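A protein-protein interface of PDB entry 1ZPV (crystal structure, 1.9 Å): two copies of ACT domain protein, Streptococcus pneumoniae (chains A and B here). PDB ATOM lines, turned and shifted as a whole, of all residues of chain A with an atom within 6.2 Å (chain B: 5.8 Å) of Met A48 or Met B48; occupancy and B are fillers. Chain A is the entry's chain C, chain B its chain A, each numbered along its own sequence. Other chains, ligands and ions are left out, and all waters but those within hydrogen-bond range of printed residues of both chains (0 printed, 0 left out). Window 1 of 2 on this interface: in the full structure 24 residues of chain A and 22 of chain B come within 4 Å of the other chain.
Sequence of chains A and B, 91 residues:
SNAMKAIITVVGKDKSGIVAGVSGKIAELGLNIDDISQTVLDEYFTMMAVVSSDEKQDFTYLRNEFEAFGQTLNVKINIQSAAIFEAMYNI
Thr A9 touches its own counterpart, Thr B9. Val A11 touches Met B48, but with the chains exchanged Met A48 does not touch Val B11 (4.7 Å). Met A48 touches Thr B9, but with the chains exchanged Thr A9 does not touch Met B48 (5.2 Å). Met A48 touches its own counterpart, Met B48. Positions printed for both chains: 7, 8, 9, 10, 11, 35, 36, 37, 38, 41, 46, 47, 48, 49 and 50.
Ile A8 touches none of the printed residues of chain B. Of the printed residues of chain B, Thr A9 touches Thr B9. Of the printed residues of chain B, Met A48 touches Thr B9, Leu B41, Thr B46 and Met B48. Printed residues of chain B within 4 Å of Ala A49: Leu B41. Ile B7 touches none of the printed residues of chain A. Of the printed residues of chain A, Thr B46 touches Met A48 (2.8 Å). Met B48 touches just these residues of chain A: Val A11, Leu A41, Thr A46 and Met A48. Printed residues of chain A within 4 Å of Val B50: Leu A41. The nearest residue of chain A that does not touch Met B48 is Val A10 (4.5 Å). The nearest printed residue of chain A that does not touch Val B50 is Thr A46 (6.4 Å).
The backbone carbonyl oxygen (O) of Val B10 lies within hydrogen-bond range of the side-chain hydroxyl (OG1) of Thr B46 (3.2 Å). The backbone NH of Val B50 lies within hydrogen-bond range of the backbone carbonyl oxygen of Asp B35, at 2.9 Å. The backbone carbonyl oxygen (O) of Met B48 is in hydrogen-bond range of the backbone NH (N) of Ser B37 (2.8 Å). The backbone NH (N) of Ile A8 sits at hydrogen-bond distance from the backbone carbonyl oxygen (O) of Ala A49, at 2.7 Å. O of Asp A35 is in hydrogen-bond range of N of Val A50 (2.9 Å). The backbone carbonyl oxygen (O) of Ser A37 lies within hydrogen-bond range of the backbone NH (N) of Met A48 (2.8 Å).
Of the 15 printed residues of chain A, 11 touch a printed residue of chain B. Printed residues of chain A that touch a printed residue of chain B: Ile A7, Thr A9, Val A11, Asp A35, Ile A36, Ser A37, Leu A41, Thr A46, Met A48, Ala A49 and Val A50. Hydrophobic or aromatic side chains of chain A that line the printed part of chain B: Ile A7, Val A11, Leu A41, Met A48 and Val A50. Printed residues of chain B that touch a printed residue of chain A: Thr B9, Val B11, Asp B35, Ile B36, Ser B37, Leu B41, Thr B46, Met B48 and Val B50. Hydrophobic or aromatic side chains of chain B within 4 Å of the printed part of chain A: Val B11, Leu B41, Met B48 and Val B50. Among the printed residues, 18 pairs touch across the chains.
Among the printed residues, merely in contact across the chains: Ile A7 with Val B11 (3.9 Å), Thr A9 with Thr B9 (3.99 Å), Val A11 with Met B48 (3.7 Å), Asp A35 with Leu B41 (3.5 Å), Ile A36 with Leu B41 (3.6 Å), Ser A37 with Leu B41 (3.9 Å), Leu A41 with Asp B35 (3.6 Å), Leu A41 with Ile B36 (3.7 Å), Leu A41 with Ser B37 (3.6 Å), Leu A41 with Met B48 (3.7 Å), Leu A41 with Val B50 (3.7 Å), Thr A46 with Met B48 (3.8 Å), Met A48 with Thr B9 (2.9 Å), Met A48 with Leu B41 (3.7 Å), Met A48 with Met B48 (3.0 Å), Ala A49 with Leu B41 (3.7 Å) and Val A50 with Leu B41 (3.6 Å).
SD of Met A48 is in hydrogen-bond range of OG1 of Thr B46 (2.8 Å).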
ATOM      1  N   ILE A   7      12.926  -3.432  27.526  1.00  0.00           N
ATOM      2  CA  ILE A   7      12.827  -2.388  26.515  1.00  0.00           C
ATOM      3  C   ILE A   7      11.388  -2.396  26.012  1.00  0.00           C
ATOM      4  O   ILE A   7      10.888  -3.435  25.616  1.00  0.00           O
ATOM      5  CB  ILE A   7      13.820  -2.628  25.336  1.00  0.00           C
ATOM      6  CG1 ILE A   7      15.283  -2.675  25.851  1.00  0.00           C
ATOM      7  CG2 ILE A   7      13.689  -1.509  24.312  1.00  0.00           C
ATOM      8  CD1 ILE A   7      15.735  -4.066  26.317  1.00  0.00           C
ATOM      9  N   ILE A   8      10.732  -1.239  26.086  1.00  0.00           N
ATOM     10  CA  ILE A   8       9.351  -1.089  25.676  1.00  0.00           C
ATOM     11  C   ILE A   8       9.325  -0.284  24.390  1.00  0.00           C
ATOM     12  O   ILE A   8       9.987   0.768  24.260  1.00  0.00           O
ATOM     13  CB  ILE A   8       8.510  -0.357  26.749  1.00  0.00           C
ATOM     14  CG1 ILE A   8       8.499  -1.144  28.063  1.00  0.00           C
ATOM     15  CG2 ILE A   8       7.067   0.003  26.219  1.00  0.00           C
ATOM     16  CD1 ILE A   8       7.645  -0.457  29.243  1.00  0.00           C
ATOM     17  N   THR A   9       8.547  -0.752  23.438  1.00  0.00           N
ATOM     18  CA  THR A   9       8.464  -0.024  22.188  1.00  0.00           C
ATOM     19  C   THR A   9       7.000   0.218  21.878  1.00  0.00           C
ATOM     20  O   THR A   9       6.120  -0.628  22.148  1.00  0.00           O
ATOM     21  CB  THR A   9       9.212  -0.751  21.043  1.00  0.00           C
ATOM     22  OG1 THR A   9       8.689  -2.047  20.890  1.00  0.00           O
ATOM     23  CG2 THR A   9      10.680  -0.927  21.387  1.00  0.00           C
ATOM     24  N   VAL A  10       6.734   1.391  21.329  1.00  0.00           N
ATOM     25  CA  VAL A  10       5.372   1.828  21.081  1.00  0.00           C
ATOM     26  C   VAL A  10       5.254   2.393  19.666  1.00  0.00           C
ATOM     27  O   VAL A  10       6.130   3.160  19.221  1.00  0.00           O
ATOM     28  CB  VAL A  10       4.958   2.963  22.101  1.00  0.00           C
ATOM     29  CG1 VAL A  10       3.547   3.452  21.797  1.00  0.00           C
ATOM     30  CG2 VAL A  10       5.127   2.496  23.564  1.00  0.00           C
ATOM     31  N   VAL A  11       4.177   2.002  18.968  1.00  0.00           N
ATOM     32  CA  VAL A  11       3.879   2.458  17.616  1.00  0.00           C
ATOM     33  C   VAL A  11       2.401   2.765  17.537  1.00  0.00           C
ATOM     34  O   VAL A  11       1.552   1.935  17.950  1.00  0.00           O
ATOM     35  CB  VAL A  11       4.152   1.381  16.512  1.00  0.00           C
ATOM     36  CG1 VAL A  11       3.883   1.998  15.080  1.00  0.00           C
ATOM     37  CG2 VAL A  11       5.536   0.849  16.606  1.00  0.00           C
ATOM     38  N   ASP A  35      15.585   5.305  30.626  1.00  0.00           N
ATOM     39  CA  ASP A  35      15.808   6.117  29.431  1.00  0.00           C
ATOM     40  C   ASP A  35      14.565   6.059  28.560  1.00  0.00           C
ATOM     41  O   ASP A  35      13.772   5.104  28.635  1.00  0.00           O
ATOM     42  CB  ASP A  35      17.026   5.646  28.602  1.00  0.00           C
ATOM     43  CG  ASP A  35      17.667   6.794  27.787  1.00  0.00           C
ATOM     44  OD1 ASP A  35      17.026   7.868  27.676  1.00  0.00           O
ATOM     45  OD2 ASP A  35      18.777   6.595  27.220  1.00  0.00           O
ATOM     46  N   ILE A  36      14.405   7.088  27.745  1.00  0.00           N
ATOM     47  CA  ILE A  36      13.204   7.213  26.879  1.00  0.00           C
ATOM     48  C   ILE A  36      13.578   8.031  25.650  1.00  0.00           C
ATOM     49  O   ILE A  36      14.518   8.876  25.679  1.00  0.00           O
ATOM     50  CB  ILE A  36      12.018   7.823  27.681  1.00  0.00           C
ATOM     51  CG1 ILE A  36      10.661   7.639  26.973  1.00  0.00           C
ATOM     52  CG2 ILE A  36      12.271   9.317  28.080  1.00  0.00           C
ATOM     53  CD1 ILE A  36       9.479   7.998  27.842  1.00  0.00           C
ATOM     54  N   SER A  37      12.866   7.768  24.561  1.00  0.00           N
ATOM     55  CA  SER A  37      13.018   8.535  23.351  1.00  0.00           C
ATOM     56  C   SER A  37      11.726   8.404  22.550  1.00  0.00           C
ATOM     57  O   SER A  37      10.994   7.430  22.696  1.00  0.00           O
ATOM     58  CB  SER A  37      14.221   8.022  22.557  1.00  0.00           C
ATOM     59  OG  SER A  37      14.538   8.849  21.443  1.00  0.00           O
ATOM     60  N   GLN A  38      11.452   9.409  21.733  1.00  0.00           N
ATOM     61  CA  GLN A  38      10.274   9.415  20.858  1.00  0.00           C
ATOM     62  C   GLN A  38      10.636   9.993  19.519  1.00  0.00           C
ATOM     63  O   GLN A  38      11.515  10.860  19.428  1.00  0.00           O
ATOM     64  CB  GLN A  38       9.126  10.244  21.426  1.00  0.00           C
ATOM     65  CG  GLN A  38       8.804  10.009  22.884  1.00  0.00           C
ATOM     66  CD  GLN A  38       9.601  10.910  23.835  1.00  0.00           C
ATOM     67  OE1 GLN A  38      10.498  10.434  24.555  1.00  0.00           O
ATOM     68  NE2 GLN A  38       9.257  12.214  23.861  1.00  0.00           N
ATOM     69  N   LEU A  41       7.909   8.792  12.709  1.00  0.00           N
ATOM     70  CA  LEU A  41       8.585   7.906  11.776  1.00  0.00           C
ATOM     71  C   LEU A  41       7.567   7.664  10.676  1.00  0.00           C
ATOM     72  O   LEU A  41       6.538   7.023  10.918  1.00  0.00           O
ATOM     73  CB  LEU A  41       8.976   6.584  12.464  1.00  0.00           C
ATOM     74  CG  LEU A  41       9.847   5.574  11.730  1.00  0.00           C
ATOM     75  CD1 LEU A  41      11.262   6.046  11.630  1.00  0.00           C
ATOM     76  CD2 LEU A  41       9.736   4.165  12.390  1.00  0.00           C
ATOM     77  N   THR A  46       6.265   7.119  17.410  1.00  0.00           N
ATOM     78  CA  THR A  46       6.932   6.000  18.030  1.00  0.00           C
ATOM     79  C   THR A  46       7.658   6.435  19.309  1.00  0.00           C
ATOM     80  O   THR A  46       8.092   7.578  19.428  1.00  0.00           O
ATOM     81  CB  THR A  46       7.955   5.363  17.094  1.00  0.00           C
ATOM     82  OG1 THR A  46       9.106   6.207  17.019  1.00  0.00           O
ATOM     83  CG2 THR A  46       7.360   5.151  15.674  1.00  0.00           C
ATOM     84  N   MET A  47       7.722   5.550  20.290  1.00  0.00           N
ATOM     85  CA  MET A  47       8.589   5.870  21.433  1.00  0.00           C
ATOM     86  C   MET A  47       9.231   4.594  21.877  1.00  0.00           C
ATOM     87  O   MET A  47       8.746   3.499  21.557  1.00  0.00           O
ATOM     88  CB  MET A  47       7.840   6.581  22.580  1.00  0.00           C
ATOM     89  CG  MET A  47       6.677   5.888  23.081  1.00  0.00           C
ATOM     90  SD  MET A  47       5.656   6.925  24.395  1.00  0.00           S
ATOM     91  CE  MET A  47       6.635   6.664  25.777  1.00  0.00           C
ATOM     92  N   MET A  48      10.332   4.732  22.582  1.00  0.00           N
ATOM     93  CA  MET A  48      10.983   3.583  23.160  1.00  0.00           C
ATOM     94  C   MET A  48      11.457   3.963  24.542  1.00  0.00           C
ATOM     95  O   MET A  48      11.827   5.132  24.779  1.00  0.00           O
ATOM     96  CB  MET A  48      12.108   3.123  22.249  1.00  0.00           C
ATOM     97  CG  MET A  48      11.576   2.478  20.964  1.00  0.00           C
ATOM     98  SD  MET A  48      12.937   1.629  19.902  1.00  0.00           S
ATOM     99  CE  MET A  48      11.948   0.407  18.930  1.00  0.00           C
ATOM    100  N   ALA A  49      11.389   3.003  25.470  1.00  0.00           N
ATOM    101  CA  ALA A  49      11.782   3.252  26.853  1.00  0.00           C
ATOM    102  C   ALA A  49      12.476   2.021  27.410  1.00  0.00           C
ATOM    103  O   ALA A  49      12.101   0.884  27.107  1.00  0.00           O
ATOM    104  CB  ALA A  49      10.593   3.612  27.740  1.00  0.00           C
ATOM    105  N   VAL A  50      13.485   2.272  28.212  1.00  0.00           N
ATOM    106  CA  VAL A  50      14.163   1.211  28.938  1.00  0.00           C
ATOM    107  C   VAL A  50      13.715   1.408  30.359  1.00  0.00           C
ATOM    108  O   VAL A  50      13.851   2.505  30.915  1.00  0.00           O
ATOM    109  CB  VAL A  50      15.712   1.283  28.818  1.00  0.00           C
ATOM    110  CG1 VAL A  50      16.411   0.358  29.880  1.00  0.00           C
ATOM    111  CG2 VAL A  50      16.167   0.880  27.416  1.00  0.00           C
ATOM    112  N   ILE B   7       6.169  -1.762   9.954  1.00  0.00           N
ATOM    113  CA  ILE B   7       7.101  -1.102  10.841  1.00  0.00           C
ATOM    114  C   ILE B   7       8.011  -2.149  11.417  1.00  0.00           C
ATOM    115  O   ILE B   7       7.535  -3.173  11.966  1.00  0.00           O
ATOM    116  CB  ILE B   7       6.408  -0.391  12.028  1.00  0.00           C
ATOM    117  CG1 ILE B   7       5.333   0.604  11.556  1.00  0.00           C
ATOM    118  CG2 ILE B   7       7.464   0.318  12.881  1.00  0.00           C
ATOM    119  CD1 ILE B   7       3.924   0.019  11.333  1.00  0.00           C
ATOM    120  N   ILE B   8       9.313  -1.888  11.339  1.00  0.00           N
ATOM    121  CA  ILE B   8      10.303  -2.865  11.767  1.00  0.00           C
ATOM    122  C   ILE B   8      10.994  -2.307  12.999  1.00  0.00           C
ATOM    123  O   ILE B   8      11.357  -1.133  13.022  1.00  0.00           O
ATOM    124  CB  ILE B   8      11.338  -3.137  10.674  1.00  0.00           C
ATOM    125  CG1 ILE B   8      10.706  -3.881   9.484  1.00  0.00           C
ATOM    126  CG2 ILE B   8      12.593  -3.864  11.244  1.00  0.00           C
ATOM    127  CD1 ILE B   8      11.727  -4.128   8.327  1.00  0.00           C
ATOM    128  N   THR B   9      11.144  -3.136  14.024  1.00  0.00           N
ATOM    129  CA  THR B   9      11.779  -2.690  15.255  1.00  0.00           C
ATOM    130  C   THR B   9      12.978  -3.573  15.521  1.00  0.00           C
ATOM    131  O   THR B   9      12.866  -4.796  15.465  1.00  0.00           O
ATOM    132  CB  THR B   9      10.806  -2.760  16.394  1.00  0.00           C
ATOM    133  OG1 THR B   9       9.608  -2.047  16.004  1.00  0.00           O
ATOM    134  CG2 THR B   9      11.406  -2.117  17.653  1.00  0.00           C
ATOM    135  N   VAL B  10      14.105  -2.945  15.856  1.00  0.00           N
ATOM    136  CA  VAL B  10      15.347  -3.682  16.105  1.00  0.00           C
ATOM    137  C   VAL B  10      15.869  -3.260  17.465  1.00  0.00           C
ATOM    138  O   VAL B  10      16.016  -2.066  17.732  1.00  0.00           O
ATOM    139  CB  VAL B  10      16.442  -3.379  15.055  1.00  0.00           C
ATOM    140  CG1 VAL B  10      17.776  -4.209  15.379  1.00  0.00           C
ATOM    141  CG2 VAL B  10      15.955  -3.713  13.636  1.00  0.00           C
ATOM    142  N   VAL B  11      16.159  -4.244  18.309  1.00  0.00           N
ATOM    143  CA  VAL B  11      16.655  -3.971  19.664  1.00  0.00           C
ATOM    144  C   VAL B  11      17.848  -4.867  19.906  1.00  0.00           C
ATOM    145  O   VAL B  11      17.804  -6.082  19.663  1.00  0.00           O
ATOM    146  CB  VAL B  11      15.575  -4.195  20.751  1.00  0.00           C
ATOM    147  CG1 VAL B  11      16.082  -3.722  22.118  1.00  0.00           C
ATOM    148  CG2 VAL B  11      14.208  -3.478  20.384  1.00  0.00           C
ATOM    149  N   ASP B  35      11.046   5.463   5.961  1.00  0.00           N
ATOM    150  CA  ASP B  35      11.694   6.267   7.028  1.00  0.00           C
ATOM    151  C   ASP B  35      12.492   5.337   7.918  1.00  0.00           C
ATOM    152  O   ASP B  35      12.218   4.124   8.003  1.00  0.00           O
ATOM    153  CB  ASP B  35      10.659   7.070   7.858  1.00  0.00           C
ATOM    154  CG  ASP B  35      11.260   8.344   8.505  1.00  0.00           C
ATOM    155  OD1 ASP B  35      12.497   8.527   8.446  1.00  0.00           O
ATOM    156  OD2 ASP B  35      10.478   9.175   9.042  1.00  0.00           O
ATOM    157  N   ILE B  36      13.479   5.897   8.602  1.00  0.00           N
ATOM    158  CA  ILE B  36      14.347   5.115   9.486  1.00  0.00           C
ATOM    159  C   ILE B  36      14.845   6.007  10.624  1.00  0.00           C
ATOM    160  O   ILE B  36      14.973   7.213  10.467  1.00  0.00           O
ATOM    161  CB  ILE B  36      15.522   4.522   8.709  1.00  0.00           C
ATOM    162  CG1 ILE B  36      16.391   3.604   9.596  1.00  0.00           C
ATOM    163  CG2 ILE B  36      16.315   5.665   7.986  1.00  0.00           C
ATOM    164  CD1 ILE B  36      16.922   2.391   8.830  1.00  0.00           C
ATOM    165  N   SER B  37      15.087   5.407  11.783  1.00  0.00           N
ATOM    166  CA  SER B  37      15.583   6.137  12.950  1.00  0.00           C
ATOM    167  C   SER B  37      16.391   5.186  13.785  1.00  0.00           C
ATOM    168  O   SER B  37      16.110   3.992  13.816  1.00  0.00           O
ATOM    169  CB  SER B  37      14.423   6.642  13.797  1.00  0.00           C
ATOM    170  OG  SER B  37      13.683   5.511  14.261  1.00  0.00           O
ATOM    171  N   GLN B  38      17.403   5.705  14.470  1.00  0.00           N
ATOM    172  CA  GLN B  38      18.230   4.870  15.316  1.00  0.00           C
ATOM    173  C   GLN B  38      18.544   5.651  16.586  1.00  0.00           C
ATOM    174  O   GLN B  38      18.767   6.871  16.539  1.00  0.00           O
ATOM    175  CB  GLN B  38      19.506   4.452  14.577  1.00  0.00           C
ATOM    176  CG  GLN B  38      20.636   5.466  14.736  1.00  0.00           C
ATOM    177  CD  GLN B  38      21.718   5.381  13.665  1.00  0.00           C
ATOM    178  OE1 GLN B  38      21.436   5.492  12.470  1.00  0.00           O
ATOM    179  NE2 GLN B  38      22.961   5.202  14.093  1.00  0.00           N
ATOM    180  N   LEU B  41      19.794   3.897  23.743  1.00  0.00           N
ATOM    181  CA  LEU B  41      18.841   4.025  24.848  1.00  0.00           C
ATOM    182  C   LEU B  41      19.362   3.187  26.000  1.00  0.00           C
ATOM    183  O   LEU B  41      19.432   1.936  25.906  1.00  0.00           O
ATOM    184  CB  LEU B  41      17.470   3.483  24.393  1.00  0.00           C
ATOM    185  CG  LEU B  41      16.203   3.913  25.126  1.00  0.00           C
ATOM    186  CD1 LEU B  41      15.936   5.381  24.907  1.00  0.00           C
ATOM    187  CD2 LEU B  41      15.028   3.057  24.725  1.00  0.00           C
ATOM    188  N   THR B  46      19.094   0.932  19.329  1.00  0.00           N
ATOM    189  CA  THR B  46      17.717   0.623  18.911  1.00  0.00           C
ATOM    190  C   THR B  46      17.445   1.227  17.539  1.00  0.00           C
ATOM    191  O   THR B  46      17.974   2.271  17.218  1.00  0.00           O
ATOM    192  CB  THR B  46      16.660   1.105  19.911  1.00  0.00           C
ATOM    193  OG1 THR B  46      15.409   0.447  19.644  1.00  0.00           O
ATOM    194  CG2 THR B  46      16.448   2.598  19.778  1.00  0.00           C
ATOM    195  N   MET B  47      16.623   0.582  16.727  1.00  0.00           N
ATOM    196  CA  MET B  47      16.459   1.067  15.369  1.00  0.00           C
ATOM    197  C   MET B  47      15.045   0.745  14.905  1.00  0.00           C
ATOM    198  O   MET B  47      14.548  -0.337  15.184  1.00  0.00           O
ATOM    199  CB  MET B  47      17.535   0.410  14.486  1.00  0.00           C
ATOM    200  CG  MET B  47      17.624   0.932  13.123  1.00  0.00           C
ATOM    201  SD  MET B  47      18.556  -0.433  12.059  1.00  0.00           S
ATOM    202  CE  MET B  47      17.411  -0.437  10.725  1.00  0.00           C
ATOM    203  N   MET B  48      14.386   1.709  14.260  1.00  0.00           N
ATOM    204  CA  MET B  48      13.074   1.476  13.676  1.00  0.00           C
ATOM    205  C   MET B  48      13.029   1.937  12.226  1.00  0.00           C
ATOM    206  O   MET B  48      13.670   2.942  11.853  1.00  0.00           O
ATOM    207  CB  MET B  48      12.007   2.156  14.510  1.00  0.00           C
ATOM    208  CG  MET B  48      11.868   1.546  15.897  1.00  0.00           C
ATOM    209  SD  MET B  48      10.516   2.325  17.051  1.00  0.00           S
ATOM    210  CE  MET B  48       9.018   1.800  16.001  1.00  0.00           C
ATOM    211  N   ALA B  49      12.351   1.173  11.385  1.00  0.00           N
ATOM    212  CA  ALA B  49      12.198   1.550   9.961  1.00  0.00           C
ATOM    213  C   ALA B  49      10.756   1.295   9.516  1.00  0.00           C
ATOM    214  O   ALA B  49      10.136   0.342   9.968  1.00  0.00           O
ATOM    215  CB  ALA B  49      13.163   0.735   9.106  1.00  0.00           C
ATOM    216  N   VAL B  50      10.197   2.189   8.720  1.00  0.00           N
ATOM    217  CA  VAL B  50       8.921   1.935   8.076  1.00  0.00           C
ATOM    218  C   VAL B  50       9.319   1.536   6.654  1.00  0.00           C
ATOM    219  O   VAL B  50      10.146   2.215   6.014  1.00  0.00           O
ATOM    220  CB  VAL B  50       8.009   3.183   8.068  1.00  0.00           C
ATOM    221  CG1 VAL B  50       6.775   3.012   7.130  1.00  0.00           C
ATOM    222  CG2 VAL B  50       7.550   3.505   9.458  1.00  0.00           C
